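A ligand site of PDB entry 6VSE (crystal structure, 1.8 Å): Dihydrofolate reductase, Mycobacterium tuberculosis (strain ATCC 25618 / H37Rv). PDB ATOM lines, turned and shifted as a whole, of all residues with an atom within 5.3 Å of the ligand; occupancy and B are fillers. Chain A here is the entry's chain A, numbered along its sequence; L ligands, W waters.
Water W6 lies within hydrogen-bond range of an oxygen (O17) of the ligand and the guanidinium group (NH1) of Arg 69. Water W4 lies within hydrogen-bond range of the side-chain hydroxyl (OG) of Ser 51 (2.7 Å) and an oxygen (O13) of the ligand (2.8 Å). Water W5 bridges OE1 of Gln 100 and NH1 of Arg 69.
O of Gly 17 sits at hydrogen-bond distance from N of Ala 128 (2.9 Å). The backbone NH (N) of Ile 16 is in hydrogen-bond range of the backbone carbonyl oxygen (O) of Ala 128 (2.8 Å). The backbone carbonyl oxygen (O) of Thr 48 is in hydrogen-bond range of the side-chain hydroxyl (OG) of Ser 51. The backbone carbonyl oxygen (O) of Ile 7 sits at hydrogen-bond distance from the side-chain hydroxyl (OH) of Tyr 102 (2.6 Å). The backbone NH (N) of Arg 46 sits at hydrogen-bond distance from the backbone carbonyl oxygen (O) of Leu 67, 3.1 Å away. The side-chain hydroxyl (OG1) of Thr 48 is in hydrogen-bond range of the backbone NH (N) of Gly 98, 3.1 Å away. OH of Tyr 102 lies close to N of Gly 97 (3.5 Å). N of Gly 45 is in hydrogen-bond range of O of Gly 97 (2.8 Å).
An oxygen (O14) of the ligand sits close to the backbone carbonyl oxygen (O) of Ala 9 (2.8 Å). O14 of the ligand sits close to O of Ile 16 (2.9 Å). The backbone carbonyl oxygen (O) of Leu 67 sits close to an oxygen (O4) of the ligand, 3.5 Å away. N4 of the ligand lies close to O of Gly 82 (3.5 Å). Trp 8 touches the ligand. Gly 17 touches the ligand. N of Arg 18 touches O12 of the ligand (3.7 Å). Gly 20 touches the ligand (C to O12, 3.2 Å). CG1 of Ile 22 touches O13 of the ligand, 3.6 Å away. CA of Gly 45 touches O3 of the ligand, at 3.3 Å. Ile 96 touches the ligand. Gly 97 touches the ligand (CA to C20, 3.8 Å). Tyr 102 touches the ligand. Leu 104 touches the ligand. Ala 128 touches the ligand. Of the 34 residues printed, 26 come within 4 Å of the ligand. The nearest printed residue that does not touch the ligand is Trp 24 (4.05 Å).
An oxygen (O9) of the ligand is in salt-bridge range of the guanidinium group (NH1) of Arg 47. The backbone NH (N) of Val 101 is in hydrogen-bond range of an oxygen (O1) of the ligand, 3.3 Å away. The backbone NH of Asp 21 sits at hydrogen-bond distance from an oxygen (O12) of the ligand (3.2 Å). O2 of the ligand sits at hydrogen-bond distance from N of Gly 98. An oxygen (O4) of the ligand lies within hydrogen-bond range of the backbone NH (N) of Arg 46, 3.4 Å away. The side-chain amide nitrogen (NE2) of Gln 70 lies within hydrogen-bond range of an oxygen (O16) of the ligand, at 2.9 Å. N of Thr 48 is in hydrogen-bond range of O2 of the ligand (3.1 Å). The side-chain hydroxyl of Thr 48 lies within hydrogen-bond range of an oxygen (O2) of the ligand (2.6 Å). O15 of the ligand is in salt-bridge range of NH2 of Arg 46 (2.8 Å). N of Gln 100 sits at hydrogen-bond distance from O8 of the ligand (2.9 Å). N of Gly 99 sits at hydrogen-bond distance from O8 of the ligand (3.0 Å). The backbone NH of Arg 69 lies within hydrogen-bond range of an oxygen (O17) of the ligand (2.8 Å). The backbone carbonyl oxygen of Asp 21 is in hydrogen-bond range of an oxygen (O12) of the ligand (2.9 Å). N of Arg 47 is in hydrogen-bond range of O3 of the ligand. O16 of the ligand is in hydrogen-bond range of OG of Ser 68, at 2.7 Å.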
ATOM      1  N   ILE A   7       7.259  29.410 -13.219  1.00  0.00           N
ATOM      2  CA  ILE A   7       7.864  28.175 -12.745  1.00  0.00           C
ATOM      3  C   ILE A   7       6.732  27.189 -12.450  1.00  0.00           C
ATOM      4  O   ILE A   7       5.761  27.542 -11.775  1.00  0.00           O
ATOM      5  CB  ILE A   7       8.780  28.427 -11.535  1.00  0.00           C
ATOM      6  CG1 ILE A   7       9.481  27.128 -11.079  1.00  0.00           C
ATOM      7  CG2 ILE A   7       8.035  29.140 -10.376  1.00  0.00           C
ATOM      8  CD1 ILE A   7      10.700  27.401 -10.160  1.00  0.00           C
ATOM      9  N   TRP A   8       6.829  25.981 -12.996  1.00  0.00           N
ATOM     10  CA  TRP A   8       5.796  24.965 -12.798  1.00  0.00           C
ATOM     11  C   TRP A   8       6.383  23.582 -13.020  1.00  0.00           C
ATOM     12  O   TRP A   8       7.455  23.421 -13.587  1.00  0.00           O
ATOM     13  CB  TRP A   8       4.587  25.196 -13.736  1.00  0.00           C
ATOM     14  CG  TRP A   8       4.715  24.763 -15.184  1.00  0.00           C
ATOM     15  CD1 TRP A   8       4.550  23.491 -15.701  1.00  0.00           C
ATOM     16  CD2 TRP A   8       4.953  25.624 -16.302  1.00  0.00           C
ATOM     17  NE1 TRP A   8       4.698  23.519 -17.069  1.00  0.00           N
ATOM     18  CE2 TRP A   8       4.931  24.813 -17.461  1.00  0.00           C
ATOM     19  CE3 TRP A   8       5.179  26.996 -16.446  1.00  0.00           C
ATOM     20  CZ2 TRP A   8       5.152  25.340 -18.728  1.00  0.00           C
ATOM     21  CZ3 TRP A   8       5.393  27.504 -17.702  1.00  0.00           C
ATOM     22  CH2 TRP A   8       5.374  26.679 -18.828  1.00  0.00           C
ATOM     23  N   ALA A   9       5.654  22.582 -12.515  1.00  0.00           N
ATOM     24  CA  ALA A   9       5.920  21.169 -12.763  1.00  0.00           C
ATOM     25  C   ALA A   9       4.709  20.586 -13.473  1.00  0.00           C
ATOM     26  O   ALA A   9       3.559  20.866 -13.086  1.00  0.00           O
ATOM     27  CB  ALA A   9       6.185  20.396 -11.462  1.00  0.00           C
ATOM     28  N   GLN A  10       4.943  19.773 -14.499  1.00  0.00           N
ATOM     29  CA  GLN A  10       3.847  19.179 -15.244  1.00  0.00           C
ATOM     30  C   GLN A  10       4.096  17.701 -15.477  1.00  0.00           C
ATOM     31  O   GLN A  10       5.233  17.247 -15.624  1.00  0.00           O
ATOM     32  CB  GLN A  10       3.670  19.880 -16.594  1.00  0.00           C
ATOM     33  CG  GLN A  10       4.883  19.726 -17.528  1.00  0.00           C
ATOM     34  CD  GLN A  10       4.616  20.327 -18.887  1.00  0.00           C
ATOM     35  OE1 GLN A  10       4.680  21.549 -19.055  1.00  0.00           O
ATOM     36  NE2 GLN A  10       4.274  19.481 -19.843  1.00  0.00           N
ATOM     37  N   ILE A  16      -0.938  20.085 -14.639  1.00  0.00           N
ATOM     38  CA  ILE A  16      -0.215  20.653 -13.513  1.00  0.00           C
ATOM     39  C   ILE A  16      -1.012  20.591 -12.217  1.00  0.00           C
ATOM     40  O   ILE A  16      -0.411  20.742 -11.143  1.00  0.00           O
ATOM     41  CB  ILE A  16       0.217  22.107 -13.787  1.00  0.00           C
ATOM     42  CG1 ILE A  16      -1.036  22.986 -14.009  1.00  0.00           C
ATOM     43  CG2 ILE A  16       1.156  22.171 -14.981  1.00  0.00           C
ATOM     44  CD1 ILE A  16      -0.766  24.478 -13.985  1.00  0.00           C
ATOM     45  N   GLY A  17      -2.321  20.397 -12.269  1.00  0.00           N
ATOM     46  CA  GLY A  17      -3.110  20.392 -11.055  1.00  0.00           C
ATOM     47  C   GLY A  17      -4.367  19.601 -11.270  1.00  0.00           C
ATOM     48  O   GLY A  17      -4.892  19.521 -12.391  1.00  0.00           O
ATOM     49  N   ARG A  18      -4.852  18.975 -10.193  1.00  0.00           N
ATOM     50  CA  ARG A  18      -6.114  18.249 -10.235  1.00  0.00           C
ATOM     51  C   ARG A  18      -6.752  18.301  -8.857  1.00  0.00           C
ATOM     52  O   ARG A  18      -6.073  18.104  -7.838  1.00  0.00           O
ATOM     53  CB  ARG A  18      -5.874  16.816 -10.689  1.00  0.00           C
ATOM     54  CG  ARG A  18      -7.061  15.894 -10.574  1.00  0.00           C
ATOM     55  CD  ARG A  18      -6.674  14.536 -11.113  1.00  0.00           C
ATOM     56  NE  ARG A  18      -6.350  14.644 -12.530  1.00  0.00           N
ATOM     57  CZ  ARG A  18      -5.881  13.654 -13.279  1.00  0.00           C
ATOM     58  NH1 ARG A  18      -5.681  12.441 -12.745  1.00  0.00           N
ATOM     59  NH2 ARG A  18      -5.622  13.874 -14.561  1.00  0.00           N
ATOM     60  N   GLY A  19      -8.054  18.576  -8.812  1.00  0.00           N
ATOM     61  CA  GLY A  19      -8.753  18.630  -7.539  1.00  0.00           C
ATOM     62  C   GLY A  19      -8.292  19.727  -6.594  1.00  0.00           C
ATOM     63  O   GLY A  19      -8.461  19.608  -5.375  1.00  0.00           O
ATOM     64  N   GLY A  20      -7.712  20.797  -7.129  1.00  0.00           N
ATOM     65  CA  GLY A  20      -7.183  21.860  -6.295  1.00  0.00           C
ATOM     66  C   GLY A  20      -5.813  21.599  -5.697  1.00  0.00           C
ATOM     67  O   GLY A  20      -5.351  22.417  -4.897  1.00  0.00           O
ATOM     68  N   ASP A  21      -5.174  20.490  -6.037  1.00  0.00           N
ATOM     69  CA  ASP A  21      -3.832  20.171  -5.537  1.00  0.00           C
ATOM     70  C   ASP A  21      -2.997  19.603  -6.691  1.00  0.00           C
ATOM     71  O   ASP A  21      -3.269  19.859  -7.869  1.00  0.00           O
ATOM     72  CB  ASP A  21      -3.899  19.185  -4.351  1.00  0.00           C
ATOM     73  CG  ASP A  21      -2.740  19.364  -3.405  1.00  0.00           C
ATOM     74  OD1 ASP A  21      -1.669  18.749  -3.662  1.00  0.00           O
ATOM     75  OD2 ASP A  21      -2.890  20.165  -2.443  1.00  0.00           O
ATOM     76  N   ILE A  22      -1.966  18.846  -6.340  1.00  0.00           N
ATOM     77  CA  ILE A  22      -1.005  18.310  -7.306  1.00  0.00           C
ATOM     78  C   ILE A  22      -0.873  16.807  -7.076  1.00  0.00           C
ATOM     79  O   ILE A  22      -0.696  16.380  -5.922  1.00  0.00           O
ATOM     80  CB  ILE A  22       0.365  19.011  -7.173  1.00  0.00           C
ATOM     81  CG1 ILE A  22       0.239  20.531  -7.378  1.00  0.00           C
ATOM     82  CG2 ILE A  22       1.362  18.405  -8.126  1.00  0.00           C
ATOM     83  CD1 ILE A  22       1.519  21.267  -7.088  1.00  0.00           C
ATOM     84  N   TRP A  24       1.391  14.572  -7.270  1.00  0.00           N
ATOM     85  CA  TRP A  24       2.728  14.047  -7.022  1.00  0.00           C
ATOM     86  C   TRP A  24       3.388  14.986  -6.032  1.00  0.00           C
ATOM     87  O   TRP A  24       2.852  16.050  -5.721  1.00  0.00           O
ATOM     88  CB  TRP A  24       3.583  13.943  -8.312  1.00  0.00           C
ATOM     89  CG  TRP A  24       3.854  15.291  -8.948  1.00  0.00           C
ATOM     90  CD1 TRP A  24       4.770  16.234  -8.555  1.00  0.00           C
ATOM     91  CD2 TRP A  24       3.144  15.857 -10.062  1.00  0.00           C
ATOM     92  NE1 TRP A  24       4.685  17.348  -9.367  1.00  0.00           N
ATOM     93  CE2 TRP A  24       3.685  17.147 -10.288  1.00  0.00           C
ATOM     94  CE3 TRP A  24       2.110  15.398 -10.884  1.00  0.00           C
ATOM     95  CZ2 TRP A  24       3.234  17.970 -11.325  1.00  0.00           C
ATOM     96  CZ3 TRP A  24       1.657  16.230 -11.904  1.00  0.00           C
ATOM     97  CH2 TRP A  24       2.212  17.503 -12.105  1.00  0.00           C
ATOM     98  N   GLY A  45      -2.345  32.690  -8.224  1.00  0.00           N
ATOM     99  CA  GLY A  45      -3.782  32.836  -8.199  1.00  0.00           C
ATOM    100  C   GLY A  45      -4.349  32.486  -6.843  1.00  0.00           C
ATOM    101  O   GLY A  45      -3.729  31.821  -6.013  1.00  0.00           O
ATOM    102  N   ARG A  46      -5.587  32.930  -6.621  1.00  0.00           N
ATOM    103  CA  ARG A  46      -6.187  32.724  -5.313  1.00  0.00           C
ATOM    104  C   ARG A  46      -6.365  31.234  -5.016  1.00  0.00           C
ATOM    105  O   ARG A  46      -6.198  30.804  -3.862  1.00  0.00           O
ATOM    106  CB  ARG A  46      -7.503  33.474  -5.212  1.00  0.00           C
ATOM    107  CG  ARG A  46      -8.113  33.492  -3.821  1.00  0.00           C
ATOM    108  CD  ARG A  46      -9.092  32.329  -3.642  1.00  0.00           C
ATOM    109  NE  ARG A  46     -10.105  32.323  -4.688  1.00  0.00           N
ATOM    110  CZ  ARG A  46     -10.853  31.276  -5.002  1.00  0.00           C
ATOM    111  NH1 ARG A  46     -10.710  30.133  -4.343  1.00  0.00           N
ATOM    112  NH2 ARG A  46     -11.753  31.359  -5.970  1.00  0.00           N
ATOM    113  N   ARG A  47      -6.678  30.438  -6.035  1.00  0.00           N
ATOM    114  CA  ARG A  47      -6.848  29.001  -5.806  1.00  0.00           C
ATOM    115  C   ARG A  47      -5.545  28.355  -5.379  1.00  0.00           C
ATOM    116  O   ARG A  47      -5.532  27.429  -4.553  1.00  0.00           O
ATOM    117  CB  ARG A  47      -7.381  28.321  -7.072  1.00  0.00           C
ATOM    118  CG  ARG A  47      -8.819  28.700  -7.433  1.00  0.00           C
ATOM    119  CD  ARG A  47      -9.243  27.899  -8.644  1.00  0.00           C
ATOM    120  NE  ARG A  47     -10.665  27.978  -8.908  1.00  0.00           N
ATOM    121  CZ  ARG A  47     -11.231  27.534 -10.031  1.00  0.00           C
ATOM    122  NH1 ARG A  47     -10.463  26.993 -10.974  1.00  0.00           N
ATOM    123  NH2 ARG A  47     -12.531  27.622 -10.212  1.00  0.00           N
ATOM    124  N   THR A  48      -4.420  28.822  -5.919  1.00  0.00           N
ATOM    125  CA  THR A  48      -3.146  28.261  -5.502  1.00  0.00           C
ATOM    126  C   THR A  48      -2.800  28.678  -4.072  1.00  0.00           C
ATOM    127  O   THR A  48      -2.300  27.865  -3.295  1.00  0.00           O
ATOM    128  CB  THR A  48      -2.065  28.653  -6.490  1.00  0.00           C
ATOM    129  OG1 THR A  48      -2.319  28.005  -7.748  1.00  0.00           O
ATOM    130  CG2 THR A  48      -0.704  28.204  -5.988  1.00  0.00           C
ATOM    131  N   SER A  51      -4.467  26.463  -1.788  1.00  0.00           N
ATOM    132  CA  SER A  51      -3.872  25.134  -1.709  1.00  0.00           C
ATOM    133  C   SER A  51      -2.711  25.075  -0.720  1.00  0.00           C
ATOM    134  O   SER A  51      -2.373  23.979  -0.241  1.00  0.00           O
ATOM    135  CB  SER A  51      -3.401  24.684  -3.098  1.00  0.00           C
ATOM    136  OG  SER A  51      -2.137  25.219  -3.435  1.00  0.00           O
ATOM    137  N   LEU A  67      -3.410  36.976  -6.689  1.00  0.00           N
ATOM    138  CA  LEU A  67      -4.291  37.618  -7.649  1.00  0.00           C
ATOM    139  C   LEU A  67      -5.710  37.137  -7.416  1.00  0.00           C
ATOM    140  O   LEU A  67      -5.962  35.930  -7.403  1.00  0.00           O
ATOM    141  CB  LEU A  67      -3.831  37.305  -9.066  1.00  0.00           C
ATOM    142  CG  LEU A  67      -4.495  37.940 -10.277  1.00  0.00           C
ATOM    143  CD1 LEU A  67      -4.280  39.450 -10.319  1.00  0.00           C
ATOM    144  CD2 LEU A  67      -3.889  37.296 -11.488  1.00  0.00           C
ATOM    145  N   SER A  68      -6.639  38.077  -7.178  1.00  0.00           N
ATOM    146  CA  SER A  68      -8.030  37.745  -6.915  1.00  0.00           C
ATOM    147  C   SER A  68      -8.918  38.871  -7.420  1.00  0.00           C
ATOM    148  O   SER A  68      -8.565  40.040  -7.287  1.00  0.00           O
ATOM    149  CB  SER A  68      -8.300  37.528  -5.422  1.00  0.00           C
ATOM    150  OG  SER A  68      -9.683  37.297  -5.175  1.00  0.00           O
ATOM    151  N   ARG A  69     -10.078  38.516  -7.968  1.00  0.00           N
ATOM    152  CA  ARG A  69     -11.082  39.520  -8.306  1.00  0.00           C
ATOM    153  C   ARG A  69     -11.949  39.910  -7.114  1.00  0.00           C
ATOM    154  O   ARG A  69     -12.821  40.782  -7.254  1.00  0.00           O
ATOM    155  CB  ARG A  69     -11.983  39.018  -9.439  1.00  0.00           C
ATOM    156  CG  ARG A  69     -11.267  38.801 -10.761  1.00  0.00           C
ATOM    157  CD  ARG A  69     -12.241  38.486 -11.880  1.00  0.00           C
ATOM    158  NE  ARG A  69     -11.537  38.228 -13.131  1.00  0.00           N
ATOM    159  CZ  ARG A  69     -11.075  37.038 -13.480  1.00  0.00           C
ATOM    160  NH1 ARG A  69     -11.241  35.995 -12.677  1.00  0.00           N
ATOM    161  NH2 ARG A  69     -10.446  36.884 -14.640  1.00  0.00           N
ATOM    162  N   GLN A  70     -11.776  39.274  -5.961  1.00  0.00           N
ATOM    163  CA  GLN A  70     -12.572  39.577  -4.776  1.00  0.00           C
ATOM    164  C   GLN A  70     -11.890  40.738  -4.067  1.00  0.00           C
ATOM    165  O   GLN A  70     -10.780  40.585  -3.550  1.00  0.00           O
ATOM    166  CB  GLN A  70     -12.696  38.389  -3.840  1.00  0.00           C
ATOM    167  CG  GLN A  70     -13.127  37.069  -4.449  1.00  0.00           C
ATOM    168  CD  GLN A  70     -13.091  35.946  -3.412  1.00  0.00           C
ATOM    169  OE1 GLN A  70     -13.579  36.109  -2.286  1.00  0.00           O
ATOM    170  NE2 GLN A  70     -12.488  34.813  -3.777  1.00  0.00           N
ATOM    171  N   PHE A  73     -11.078  39.849  -0.421  1.00  0.00           N
ATOM    172  CA  PHE A  73     -10.372  38.621  -0.081  1.00  0.00           C
ATOM    173  C   PHE A  73      -9.139  38.924   0.750  1.00  0.00           C
ATOM    174  O   PHE A  73      -8.310  39.754   0.378  1.00  0.00           O
ATOM    175  CB  PHE A  73      -9.972  37.844  -1.331  1.00  0.00           C
ATOM    176  CG  PHE A  73      -9.325  36.512  -1.017  1.00  0.00           C
ATOM    177  CD1 PHE A  73     -10.110  35.398  -0.794  1.00  0.00           C
ATOM    178  CD2 PHE A  73      -7.955  36.392  -0.925  1.00  0.00           C
ATOM    179  CE1 PHE A  73      -9.539  34.177  -0.489  1.00  0.00           C
ATOM    180  CE2 PHE A  73      -7.363  35.167  -0.614  1.00  0.00           C
ATOM    181  CZ  PHE A  73      -8.163  34.072  -0.393  1.00  0.00           C
ATOM    182  N   VAL A  81      -3.934  41.503  -4.954  1.00  0.00           N
ATOM    183  CA  VAL A  81      -4.081  42.482  -6.023  1.00  0.00           C
ATOM    184  C   VAL A  81      -5.164  42.013  -6.989  1.00  0.00           C
ATOM    185  O   VAL A  81      -5.460  40.817  -7.109  1.00  0.00           O
ATOM    186  CB  VAL A  81      -2.770  42.758  -6.786  1.00  0.00           C
ATOM    187  CG1 VAL A  81      -1.704  43.305  -5.824  1.00  0.00           C
ATOM    188  CG2 VAL A  81      -2.285  41.514  -7.515  1.00  0.00           C
ATOM    189  N   GLY A  82      -5.768  42.970  -7.680  1.00  0.00           N
ATOM    190  CA  GLY A  82      -6.825  42.657  -8.622  1.00  0.00           C
ATOM    191  C   GLY A  82      -6.356  42.534 -10.051  1.00  0.00           C
ATOM    192  O   GLY A  82      -7.110  42.106 -10.936  1.00  0.00           O
ATOM    193  N   SER A  83      -5.109  42.916 -10.318  1.00  0.00           N
ATOM    194  CA  SER A  83      -4.531  42.811 -11.646  1.00  0.00           C
ATOM    195  C   SER A  83      -3.067  42.404 -11.538  1.00  0.00           C
ATOM    196  O   SER A  83      -2.397  42.704 -10.560  1.00  0.00           O
ATOM    197  CB  SER A  83      -4.644  44.140 -12.419  1.00  0.00           C
ATOM    198  OG  SER A  83      -3.614  45.026 -12.058  1.00  0.00           O
ATOM    199  N   ILE A  96       3.936  31.605  -9.861  1.00  0.00           N
ATOM    200  CA  ILE A  96       4.057  30.243  -9.340  1.00  0.00           C
ATOM    201  C   ILE A  96       2.754  29.473  -9.491  1.00  0.00           C
ATOM    202  O   ILE A  96       2.593  28.408  -8.889  1.00  0.00           O
ATOM    203  CB  ILE A  96       4.556  30.254  -7.893  1.00  0.00           C
ATOM    204  CG1 ILE A  96       3.500  30.846  -6.940  1.00  0.00           C
ATOM    205  CG2 ILE A  96       5.824  31.088  -7.800  1.00  0.00           C
ATOM    206  CD1 ILE A  96       3.797  30.523  -5.467  1.00  0.00           C
ATOM    207  N   GLY A  97       1.821  29.979 -10.290  1.00  0.00           N
ATOM    208  CA  GLY A  97       0.613  29.243 -10.640  1.00  0.00           C
ATOM    209  C   GLY A  97      -0.670  29.936 -10.213  1.00  0.00           C
ATOM    210  O   GLY A  97      -0.598  30.982  -9.600  1.00  0.00           O
ATOM    211  N   GLY A  98      -1.831  29.356 -10.511  1.00  0.00           N
ATOM    212  CA  GLY A  98      -1.912  28.073 -11.202  1.00  0.00           C
ATOM    213  C   GLY A  98      -2.171  28.228 -12.683  1.00  0.00           C
ATOM    214  O   GLY A  98      -1.660  29.150 -13.324  1.00  0.00           O
ATOM    215  N   GLY A  99      -2.984  27.328 -13.231  1.00  0.00           N
ATOM    216  CA  GLY A  99      -3.207  27.320 -14.675  1.00  0.00           C
ATOM    217  C   GLY A  99      -3.680  28.654 -15.229  1.00  0.00           C
ATOM    218  O   GLY A  99      -3.188  29.116 -16.261  1.00  0.00           O
ATOM    219  N   GLN A 100      -4.643  29.290 -14.553  1.00  0.00           N
ATOM    220  CA  GLN A 100      -5.181  30.546 -15.054  1.00  0.00           C
ATOM    221  C   GLN A 100      -4.137  31.650 -15.031  1.00  0.00           C
ATOM    222  O   GLN A 100      -4.049  32.447 -15.976  1.00  0.00           O
ATOM    223  CB  GLN A 100      -6.408  30.991 -14.247  1.00  0.00           C
ATOM    224  CG  GLN A 100      -7.573  30.016 -14.273  1.00  0.00           C
ATOM    225  CD  GLN A 100      -8.779  30.549 -13.543  1.00  0.00           C
ATOM    226  OE1 GLN A 100      -8.836  31.717 -13.181  1.00  0.00           O
ATOM    227  NE2 GLN A 100      -9.763  29.680 -13.324  1.00  0.00           N
ATOM    228  N   VAL A 101      -3.363  31.716 -13.962  1.00  0.00           N
ATOM    229  CA  VAL A 101      -2.411  32.817 -13.820  1.00  0.00           C
ATOM    230  C   VAL A 101      -1.198  32.618 -14.712  1.00  0.00           C
ATOM    231  O   VAL A 101      -0.617  33.596 -15.201  1.00  0.00           O
ATOM    232  CB  VAL A 101      -2.036  33.015 -12.342  1.00  0.00           C
ATOM    233  CG1 VAL A 101      -0.909  34.022 -12.199  1.00  0.00           C
ATOM    234  CG2 VAL A 101      -3.266  33.514 -11.581  1.00  0.00           C
ATOM    235  N   TYR A 102      -0.783  31.364 -14.957  1.00  0.00           N
ATOM    236  CA  TYR A 102       0.240  31.101 -15.955  1.00  0.00           C
ATOM    237  C   TYR A 102      -0.170  31.652 -17.304  1.00  0.00           C
ATOM    238  O   TYR A 102       0.605  32.358 -17.973  1.00  0.00           O
ATOM    239  CB  TYR A 102       0.536  29.599 -16.072  1.00  0.00           C
ATOM    240  CG  TYR A 102       1.281  28.972 -14.914  1.00  0.00           C
ATOM    241  CD1 TYR A 102       2.334  29.618 -14.279  1.00  0.00           C
ATOM    242  CD2 TYR A 102       0.907  27.714 -14.458  1.00  0.00           C
ATOM    243  CE1 TYR A 102       3.000  29.023 -13.212  1.00  0.00           C
ATOM    244  CE2 TYR A 102       1.564  27.111 -13.399  1.00  0.00           C
ATOM    245  CZ  TYR A 102       2.609  27.752 -12.786  1.00  0.00           C
ATOM    246  OH  TYR A 102       3.231  27.122 -11.739  1.00  0.00           O
ATOM    247  N   LEU A 104      -2.352  33.980 -17.954  1.00  0.00           N
ATOM    248  CA  LEU A 104      -2.453  35.434 -17.864  1.00  0.00           C
ATOM    249  C   LEU A 104      -1.089  36.118 -17.900  1.00  0.00           C
ATOM    250  O   LEU A 104      -0.946  37.215 -18.466  1.00  0.00           O
ATOM    251  CB  LEU A 104      -3.195  35.816 -16.578  1.00  0.00           C
ATOM    252  CG  LEU A 104      -3.447  37.303 -16.351  1.00  0.00           C
ATOM    253  CD1 LEU A 104      -4.642  37.745 -17.158  1.00  0.00           C
ATOM    254  CD2 LEU A 104      -3.669  37.560 -14.877  1.00  0.00           C
ATOM    255  N   ALA A 128      -6.000  21.544 -14.174  1.00  0.00           N
ATOM    256  CA  ALA A 128      -5.236  22.705 -14.596  1.00  0.00           C
ATOM    257  C   ALA A 128      -4.086  22.244 -15.476  1.00  0.00           C
ATOM    258  O   ALA A 128      -3.484  21.202 -15.243  1.00  0.00           O
ATOM    259  CB  ALA A 128      -4.691  23.473 -13.384  1.00  0.00           C
HETATM  260  P1  LIG L   1      -5.267  29.687 -10.031  1.00  0.00           P
HETATM  261  O1  LIG L   1      -4.735  30.148 -11.355  1.00  0.00           O
HETATM  262  O2  LIG L   1      -4.327  29.193  -8.977  1.00  0.00           O
HETATM  263  O3  LIG L   1      -6.169  30.871  -9.287  1.00  0.00           O
HETATM  264  C1  LIG L   1      -7.298  31.157 -10.093  1.00  0.00           C
HETATM  265  C2  LIG L   1      -7.889  32.420  -9.427  1.00  0.00           C
HETATM  266  O4  LIG L   1      -7.003  33.495  -9.670  1.00  0.00           O
HETATM  267  C3  LIG L   1      -9.286  32.847  -9.967  1.00  0.00           C
HETATM  268  O5  LIG L   1     -10.309  32.103  -9.345  1.00  0.00           O
HETATM  269  C4  LIG L   1      -9.265  34.303  -9.419  1.00  0.00           C
HETATM  270  O6  LIG L   1      -9.331  34.364  -8.109  1.00  0.00           O
HETATM  271  C5  LIG L   1      -7.781  34.680  -9.756  1.00  0.00           C
HETATM  272  N1  LIG L   1      -7.661  35.242 -11.083  1.00  0.00           N
HETATM  273  C6  LIG L   1      -7.524  34.589 -12.296  1.00  0.00           C
HETATM  274  N2  LIG L   1      -7.465  35.427 -13.353  1.00  0.00           N
HETATM  275  C7  LIG L   1      -7.577  36.699 -12.779  1.00  0.00           C
HETATM  276  C8  LIG L   1      -7.578  37.988 -13.320  1.00  0.00           C
HETATM  277  N3  LIG L   1      -7.455  38.173 -14.683  1.00  0.00           N
HETATM  278  N4  LIG L   1      -7.705  39.097 -12.527  1.00  0.00           N
HETATM  279  C9  LIG L   1      -7.823  38.843 -11.179  1.00  0.00           C
HETATM  280  N5  LIG L   1      -7.828  37.678 -10.503  1.00  0.00           N
HETATM  281  C10 LIG L   1      -7.698  36.596 -11.349  1.00  0.00           C
HETATM  282  O7  LIG L   1      -6.482  28.615 -10.372  1.00  0.00           O
HETATM  283  P2  LIG L   1      -6.221  27.269 -11.235  1.00  0.00           P
HETATM  284  O8  LIG L   1      -5.935  27.599 -12.655  1.00  0.00           O
HETATM  285  O9  LIG L   1      -7.322  26.287 -10.926  1.00  0.00           O
HETATM  286  O10 LIG L   1      -4.784  26.437 -10.766  1.00  0.00           O
HETATM  287  C11 LIG L   1      -4.934  25.827  -9.520  1.00  0.00           C
HETATM  288  C12 LIG L   1      -4.355  24.432  -9.664  1.00  0.00           C
HETATM  289  O11 LIG L   1      -2.976  24.542 -10.074  1.00  0.00           O
HETATM  290  C13 LIG L   1      -4.351  23.681  -8.295  1.00  0.00           C
HETATM  291  O12 LIG L   1      -4.520  22.334  -8.575  1.00  0.00           O
HETATM  292  C14 LIG L   1      -2.923  23.893  -7.832  1.00  0.00           C
HETATM  293  O13 LIG L   1      -2.495  22.850  -6.992  1.00  0.00           O
HETATM  294  C15 LIG L   1      -2.224  23.750  -9.203  1.00  0.00           C
HETATM  295  N6  LIG L   1      -0.829  24.244  -9.186  1.00  0.00           N
HETATM  296  C16 LIG L   1       0.157  23.459  -9.764  1.00  0.00           C
HETATM  297  C17 LIG L   1       1.444  23.890  -9.806  1.00  0.00           C
HETATM  298  C18 LIG L   1       2.408  23.020 -10.430  1.00  0.00           C
HETATM  299  O14 LIG L   1       2.200  21.847 -10.802  1.00  0.00           O
HETATM  300  N7  LIG L   1       3.641  23.555 -10.592  1.00  0.00           N
HETATM  301  C19 LIG L   1       1.868  25.200  -9.227  1.00  0.00           C
HETATM  302  C20 LIG L   1       0.739  25.982  -8.680  1.00  0.00           C
HETATM  303  C21 LIG L   1      -0.511  25.520  -8.660  1.00  0.00           C
HETATM  304  P3  LIG L   1     -10.945  34.704  -7.385  1.00  0.00           P
HETATM  305  O15 LIG L   1     -11.668  33.452  -7.793  1.00  0.00           O
HETATM  306  O16 LIG L   1     -10.575  34.832  -5.901  1.00  0.00           O
HETATM  307  O17 LIG L   1     -11.287  35.958  -8.120  1.00  0.00           O
HETATM  308  O   HOH W   1      -6.901  21.527  -9.870  1.00  0.00           O
HETATM  309  O   HOH W   2      -7.668  24.122  -9.749  1.00  0.00           O
HETATM  310  O   HOH W   3      -7.524  35.100 -16.087  1.00  0.00           O
HETATM  311  O   HOH W   4      -0.590  23.853  -5.187  1.00  0.00           O
HETATM  312  O   HOH W   5     -10.477  33.457 -13.502  1.00  0.00           O
HETATM  313  O   HOH W   6     -12.666  35.621 -10.332  1.00  0.00           O
HETATM  314  O   HOH W   7      -7.006  26.071 -14.594  1.00  0.00           O
